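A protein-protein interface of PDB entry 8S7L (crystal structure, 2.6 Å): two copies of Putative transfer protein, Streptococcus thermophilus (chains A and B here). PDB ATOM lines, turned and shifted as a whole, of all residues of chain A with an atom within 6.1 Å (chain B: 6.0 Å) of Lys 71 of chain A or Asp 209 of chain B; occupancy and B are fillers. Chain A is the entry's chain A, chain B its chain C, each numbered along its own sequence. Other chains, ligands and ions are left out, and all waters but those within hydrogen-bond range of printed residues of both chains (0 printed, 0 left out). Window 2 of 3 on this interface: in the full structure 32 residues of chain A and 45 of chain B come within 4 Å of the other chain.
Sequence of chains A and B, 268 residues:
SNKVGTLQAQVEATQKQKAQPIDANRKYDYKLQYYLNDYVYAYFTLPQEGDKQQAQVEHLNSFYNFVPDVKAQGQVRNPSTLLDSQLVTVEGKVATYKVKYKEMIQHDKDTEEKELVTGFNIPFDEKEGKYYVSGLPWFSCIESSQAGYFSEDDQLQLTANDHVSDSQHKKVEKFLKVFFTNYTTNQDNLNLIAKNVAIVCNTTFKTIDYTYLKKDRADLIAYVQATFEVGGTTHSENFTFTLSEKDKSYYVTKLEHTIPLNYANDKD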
ATOM      1  N   ASP A  69       9.351 -23.288  17.991  1.00  0.00           N
ATOM      2  CA  ASP A  69       9.570 -22.994  19.386  1.00  0.00           C
ATOM      3  C   ASP A  69      10.732 -23.870  19.855  1.00  0.00           C
ATOM      4  O   ASP A  69      10.611 -25.093  19.847  1.00  0.00           O
ATOM      5  CB  ASP A  69       8.235 -23.177  20.106  1.00  0.00           C
ATOM      6  CG  ASP A  69       8.152 -22.966  21.608  1.00  0.00           C
ATOM      7  OD1 ASP A  69       9.175 -22.580  22.173  1.00  0.00           O
ATOM      8  OD2 ASP A  69       7.093 -23.285  22.166  1.00  0.00           O
ATOM      9  N   VAL A  70      11.822 -23.206  20.243  1.00  0.00           N
ATOM     10  CA  VAL A  70      13.074 -23.847  20.607  1.00  0.00           C
ATOM     11  C   VAL A  70      13.443 -23.473  22.041  1.00  0.00           C
ATOM     12  O   VAL A  70      13.721 -22.321  22.257  1.00  0.00           O
ATOM     13  CB  VAL A  70      14.171 -23.380  19.648  1.00  0.00           C
ATOM     14  CG1 VAL A  70      15.547 -23.775  20.133  1.00  0.00           C
ATOM     15  CG2 VAL A  70      13.926 -23.920  18.239  1.00  0.00           C
ATOM     16  N   LYS A  71      13.474 -24.408  22.993  1.00  0.00           N
ATOM     17  CA  LYS A  71      13.862 -24.050  24.355  1.00  0.00           C
ATOM     18  C   LYS A  71      15.342 -23.697  24.476  1.00  0.00           C
ATOM     19  O   LYS A  71      15.630 -22.781  25.204  1.00  0.00           O
ATOM     20  CB  LYS A  71      13.528 -25.047  25.446  1.00  0.00           C
ATOM     21  CG  LYS A  71      12.103 -25.594  25.347  1.00  0.00           C
ATOM     22  CD  LYS A  71      10.883 -24.684  25.172  1.00  0.00           C
ATOM     23  CE  LYS A  71      10.311 -24.176  26.433  1.00  0.00           C
ATOM     24  NZ  LYS A  71       9.090 -23.464  26.040  1.00  0.00           N
ATOM     25  N   ALA A  72      16.261 -24.409  23.840  1.00  0.00           N
ATOM     26  CA  ALA A  72      17.705 -24.152  23.947  1.00  0.00           C
ATOM     27  C   ALA A  72      18.083 -22.667  23.908  1.00  0.00           C
ATOM     28  O   ALA A  72      17.539 -21.896  23.153  1.00  0.00           O
ATOM     29  CB  ALA A  72      18.473 -24.861  22.840  1.00  0.00           C
ATOM     30  N   GLN A  73      19.017 -22.251  24.754  1.00  0.00           N
ATOM     31  CA  GLN A  73      19.280 -20.823  24.914  1.00  0.00           C
ATOM     32  C   GLN A  73      19.885 -20.226  23.642  1.00  0.00           C
ATOM     33  O   GLN A  73      19.233 -19.443  22.971  1.00  0.00           O
ATOM     34  CB  GLN A  73      20.243 -20.490  26.058  1.00  0.00           C
ATOM     35  CG  GLN A  73      19.647 -20.629  27.456  1.00  0.00           C
ATOM     36  CD  GLN A  73      18.335 -19.891  27.624  1.00  0.00           C
ATOM     37  OE1 GLN A  73      17.914 -19.097  26.770  1.00  0.00           O
ATOM     38  NE2 GLN A  73      17.666 -20.160  28.737  1.00  0.00           N
ATOM     39  N   GLN A  75      22.060 -21.561  20.423  1.00  0.00           N
ATOM     40  CA  GLN A  75      22.702 -22.444  19.455  1.00  0.00           C
ATOM     41  C   GLN A  75      23.972 -21.784  18.905  1.00  0.00           C
ATOM     42  O   GLN A  75      24.030 -20.565  18.878  1.00  0.00           O
ATOM     43  CB  GLN A  75      21.745 -22.785  18.310  1.00  0.00           C
ATOM     44  CG  GLN A  75      20.353 -23.306  18.713  1.00  0.00           C
ATOM     45  CD  GLN A  75      20.244 -24.698  19.347  1.00  0.00           C
ATOM     46  OE1 GLN A  75      21.193 -25.311  19.867  1.00  0.00           O
ATOM     47  NE2 GLN A  75      19.020 -25.219  19.354  1.00  0.00           N
ATOM     48  N   GLN B 157       2.987 -24.588  20.332  1.00  0.00           N
ATOM     49  CA  GLN B 157       3.502 -24.003  21.553  1.00  0.00           C
ATOM     50  C   GLN B 157       3.863 -25.106  22.535  1.00  0.00           C
ATOM     51  O   GLN B 157       2.989 -25.860  22.958  1.00  0.00           O
ATOM     52  CB  GLN B 157       2.512 -22.948  22.063  1.00  0.00           C
ATOM     53  CG  GLN B 157       2.847 -21.524  21.609  1.00  0.00           C
ATOM     54  CD  GLN B 157       4.323 -21.197  21.795  1.00  0.00           C
ATOM     55  OE1 GLN B 157       4.782 -20.887  22.909  1.00  0.00           O
ATOM     56  NE2 GLN B 157       5.093 -21.295  20.709  1.00  0.00           N
ATOM     57  N   LEU B 158       5.153 -25.179  22.897  1.00  0.00           N
ATOM     58  CA  LEU B 158       5.681 -26.183  23.819  1.00  0.00           C
ATOM     59  C   LEU B 158       5.751 -25.599  25.221  1.00  0.00           C
ATOM     60  O   LEU B 158       6.822 -25.399  25.797  1.00  0.00           O
ATOM     61  CB  LEU B 158       7.091 -26.628  23.447  1.00  0.00           C
ATOM     62  CG  LEU B 158       7.239 -27.358  22.126  1.00  0.00           C
ATOM     63  CD1 LEU B 158       8.678 -27.851  22.130  1.00  0.00           C
ATOM     64  CD2 LEU B 158       6.126 -28.451  22.070  1.00  0.00           C
ATOM     65  N   THR B 159       4.586 -25.362  25.775  1.00  0.00           N
ATOM     66  CA  THR B 159       4.491 -24.789  27.093  1.00  0.00           C
ATOM     67  C   THR B 159       3.349 -25.570  27.665  1.00  0.00           C
ATOM     68  O   THR B 159       2.208 -25.473  27.218  1.00  0.00           O
ATOM     69  CB  THR B 159       4.193 -23.288  27.089  1.00  0.00           C
ATOM     70  OG1 THR B 159       3.086 -23.261  26.179  1.00  0.00           O
ATOM     71  CG2 THR B 159       5.395 -22.426  26.715  1.00  0.00           C
ATOM     72  N   THR B 207      21.738 -32.180  25.049  1.00  0.00           N
ATOM     73  CA  THR B 207      20.848 -31.848  26.157  1.00  0.00           C
ATOM     74  C   THR B 207      19.412 -32.218  25.816  1.00  0.00           C
ATOM     75  O   THR B 207      18.929 -32.034  24.710  1.00  0.00           O
ATOM     76  CB  THR B 207      20.905 -30.359  26.540  1.00  0.00           C
ATOM     77  OG1 THR B 207      20.503 -29.487  25.480  1.00  0.00           O
ATOM     78  CG2 THR B 207      22.307 -29.874  26.847  1.00  0.00           C
ATOM     79  N   ILE B 208      18.679 -32.618  26.831  1.00  0.00           N
ATOM     80  CA  ILE B 208      17.236 -32.651  26.724  1.00  0.00           C
ATOM     81  C   ILE B 208      16.788 -31.274  27.175  1.00  0.00           C
ATOM     82  O   ILE B 208      17.250 -30.837  28.215  1.00  0.00           O
ATOM     83  CB  ILE B 208      16.703 -33.807  27.594  1.00  0.00           C
ATOM     84  CG1 ILE B 208      17.337 -35.153  27.137  1.00  0.00           C
ATOM     85  CG2 ILE B 208      15.168 -33.839  27.628  1.00  0.00           C
ATOM     86  CD1 ILE B 208      17.415 -36.225  28.203  1.00  0.00           C
ATOM     87  N   ASP B 209      15.946 -30.594  26.393  1.00  0.00           N
ATOM     88  CA  ASP B 209      15.541 -29.244  26.734  1.00  0.00           C
ATOM     89  C   ASP B 209      14.071 -29.209  27.077  1.00  0.00           C
ATOM     90  O   ASP B 209      13.595 -28.180  27.485  1.00  0.00           O
ATOM     91  CB  ASP B 209      15.699 -28.263  25.587  1.00  0.00           C
ATOM     92  CG  ASP B 209      17.026 -28.397  24.859  1.00  0.00           C
ATOM     93  OD1 ASP B 209      17.998 -28.910  25.518  1.00  0.00           O
ATOM     94  OD2 ASP B 209      17.049 -28.015  23.641  1.00  0.00           O
ATOM     95  N   TYR B 210      13.304 -30.262  26.803  1.00  0.00           N
ATOM     96  CA  TYR B 210      11.869 -30.142  27.074  1.00  0.00           C
ATOM     97  C   TYR B 210      11.266 -31.534  27.046  1.00  0.00           C
ATOM     98  O   TYR B 210      11.796 -32.390  26.344  1.00  0.00           O
ATOM     99  CB  TYR B 210      11.096 -29.341  26.027  1.00  0.00           C
ATOM    100  CG  TYR B 210       9.584 -29.393  26.173  1.00  0.00           C
ATOM    101  CD1 TYR B 210       8.952 -28.538  27.072  1.00  0.00           C
ATOM    102  CD2 TYR B 210       8.784 -30.221  25.374  1.00  0.00           C
ATOM    103  CE1 TYR B 210       7.567 -28.543  27.226  1.00  0.00           C
ATOM    104  CE2 TYR B 210       7.393 -30.231  25.522  1.00  0.00           C
ATOM    105  CZ  TYR B 210       6.786 -29.399  26.460  1.00  0.00           C
ATOM    106  OH  TYR B 210       5.445 -29.272  26.658  1.00  0.00           O
ATOM    107  N   THR B 211      10.203 -31.742  27.823  1.00  0.00           N
ATOM    108  CA  THR B 211       9.613 -33.062  27.998  1.00  0.00           C
ATOM    109  C   THR B 211       8.245 -32.928  28.653  1.00  0.00           C
ATOM    110  O   THR B 211       8.162 -32.645  29.851  1.00  0.00           O
ATOM    111  CB  THR B 211      10.459 -33.986  28.887  1.00  0.00           C
ATOM    112  OG1 THR B 211      11.786 -34.261  28.406  1.00  0.00           O
ATOM    113  CG2 THR B 211       9.671 -35.279  29.054  1.00  0.00           C
ATOM    114  N   GLN B 225      12.155 -32.446  23.210  1.00  0.00           N
ATOM    115  CA  GLN B 225      12.980 -31.654  22.337  1.00  0.00           C
ATOM    116  C   GLN B 225      14.360 -31.771  22.923  1.00  0.00           C
ATOM    117  O   GLN B 225      14.499 -31.701  24.135  1.00  0.00           O
ATOM    118  CB  GLN B 225      12.622 -30.177  22.196  1.00  0.00           C
ATOM    119  CG  GLN B 225      13.614 -29.408  21.323  1.00  0.00           C
ATOM    120  CD  GLN B 225      13.505 -27.892  21.387  1.00  0.00           C
ATOM    121  OE1 GLN B 225      14.460 -27.165  21.779  1.00  0.00           O
ATOM    122  NE2 GLN B 225      12.335 -27.435  20.943  1.00  0.00           N
ATOM    123  N   ALA B 226      15.340 -31.941  22.036  1.00  0.00           N
ATOM    124  CA  ALA B 226      16.706 -32.162  22.446  1.00  0.00           C
ATOM    125  C   ALA B 226      17.637 -31.527  21.419  1.00  0.00           C
ATOM    126  O   ALA B 226      17.187 -31.127  20.357  1.00  0.00           O
ATOM    127  CB  ALA B 226      16.948 -33.651  22.533  1.00  0.00           C
ATOM    128  N   THR B 227      18.938 -31.642  21.685  1.00  0.00           N
ATOM    129  CA  THR B 227      19.960 -30.771  21.163  1.00  0.00           C
ATOM    130  C   THR B 227      21.150 -31.634  20.795  1.00  0.00           C
ATOM    131  O   THR B 227      21.684 -32.352  21.637  1.00  0.00           O
ATOM    132  CB  THR B 227      20.328 -29.702  22.198  1.00  0.00           C
ATOM    133  OG1 THR B 227      19.152 -28.918  22.447  1.00  0.00           O
ATOM    134  CG2 THR B 227      21.473 -28.821  21.719  1.00  0.00           C
ATOM    135  N   SER B 236      18.419 -28.075  17.640  1.00  0.00           N
ATOM    136  CA  SER B 236      17.296 -28.697  18.306  1.00  0.00           C
ATOM    137  C   SER B 236      16.508 -29.553  17.309  1.00  0.00           C
ATOM    138  O   SER B 236      16.407 -29.186  16.150  1.00  0.00           O
ATOM    139  CB  SER B 236      16.387 -27.628  18.901  1.00  0.00           C
ATOM    140  OG  SER B 236      16.907 -27.057  20.101  1.00  0.00           O
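No position is printed for both chains.
Of chain B, only Leu 158, Thr 159, Asp 209, Tyr 210 and Gln 225 come within 4 Å of Lys 71 of chain A.
Of the printed residues of chain B, Ala 72 of chain A touches Asp 209 (3.6 Å), Gln 225 (3.9 Å) and Ser 236 (3.8 Å).
Gln 73 of chain A touches none of the printed residues of chain B.
Of the printed residues of chain A, Thr 159 of chain B touches Lys 71 (3.9 Å).
Of chain A, only Lys 71 and Ala 72 come within 4 Å of Asp 209 of chain B.
Thr 211 of chain B touches none of the printed residues of chain A.
Of the printed residues of chain A, Thr 227 of chain B touches Gln 75 (3.98 Å).
The nearest residue of chain B that does not touch Lys 71 of chain A is Ser 236 of chain B (5.2 Å).
The nearest residue of chain A that does not touch Asp 209 of chain B is Gln 75 of chain A (5.5 Å).
The side-chain amino group of Lys 71 of chain A lies within salt-bridge range of the side-chain carboxylate of Asp 69 of chain A (3.97 Å).
The side-chain hydroxyl (OG1) of Thr 207 of chain B is in hydrogen-bond range of the side-chain carboxylate (OD1) of Asp 209 of chain B.
N of Asp 209 of chain B is in hydrogen-bond range of O of Gln 225 of chain B (2.9 Å).
The side-chain carboxylate (OD2) of Asp 209 of chain B is in hydrogen-bond range of the side-chain hydroxyl (OG1) of Thr 227 of chain B, at 2.6 Å.
The backbone carbonyl oxygen (O) of Tyr 210 of chain B sits at hydrogen-bond distance from the backbone NH (N) of Gln 225 of chain B, 3.2 Å away.
The side-chain hydroxyl (OG) of Ser 236 of chain B lies within hydrogen-bond range of the side-chain amide oxygen (OE1) of Gln 225 of chain B (3.0 Å).
Hydrophobic or aromatic side chains of chain A within 4 Å of the printed part of chain B: Val 70 and Ala 72.
Printed residues of chain B that touch a printed residue of chain A: Gln 157, Leu 158, Thr 159, Asp 209, Tyr 210, Gln 225, Thr 227 and Ser 236.
Along chain B the printed residues that touch a printed residue of chain A span positions 157 to 236.
The side-chain amide nitrogen of Gln 157 of chain B lies within hydrogen-bond range of the side-chain carboxylate of Asp 69 of chain A (3.2 Å).
The side-chain carboxylate (OD2) of Asp 69 of chain A is in hydrogen-bond range of the backbone NH (N) of Leu 158 of chain B (2.8 Å).
The side-chain amide nitrogen of Gln 225 of chain B sits at hydrogen-bond distance from the backbone carbonyl oxygen of Asp 69 of chain A (3.1 Å).
The side-chain amino group (NZ) of Lys 71 of chain A sits at hydrogen-bond distance from the backbone carbonyl oxygen (O) of Leu 158 of chain B, at 3.0 Å.
N of Lys 71 of chain A lies within hydrogen-bond range of OE1 of Gln 225 of chain B (3.2 Å).
NE2 of Gln 75 of chain A is in hydrogen-bond range of OG of Ser 236 of chain B, 2.9 Å away.
Gln 225 of chain B touches Val 70 of chain A.
Ser 236 of chain B touches Val 70 of chain A (OG to CG1, 3.6 Å).
Lys 71 of chain A touches Thr 159 of chain B.
CG of Lys 71 of chain A touches O of Asp 209 of chain B, 3.7 Å away.
CB of Tyr 210 of chain B touches CG of Lys 71 of chain A, 3.9 Å away.
Ala 72 of chain A touches Asp 209 of chain B.
N of Ala 72 of chain A touches OE1 of Gln 225 of chain B (3.9 Å).
Ala 72 of chain A touches Ser 236 of chain B (CB to OG, 3.8 Å).
Gln 75 of chain A touches Thr 227 of chain B.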
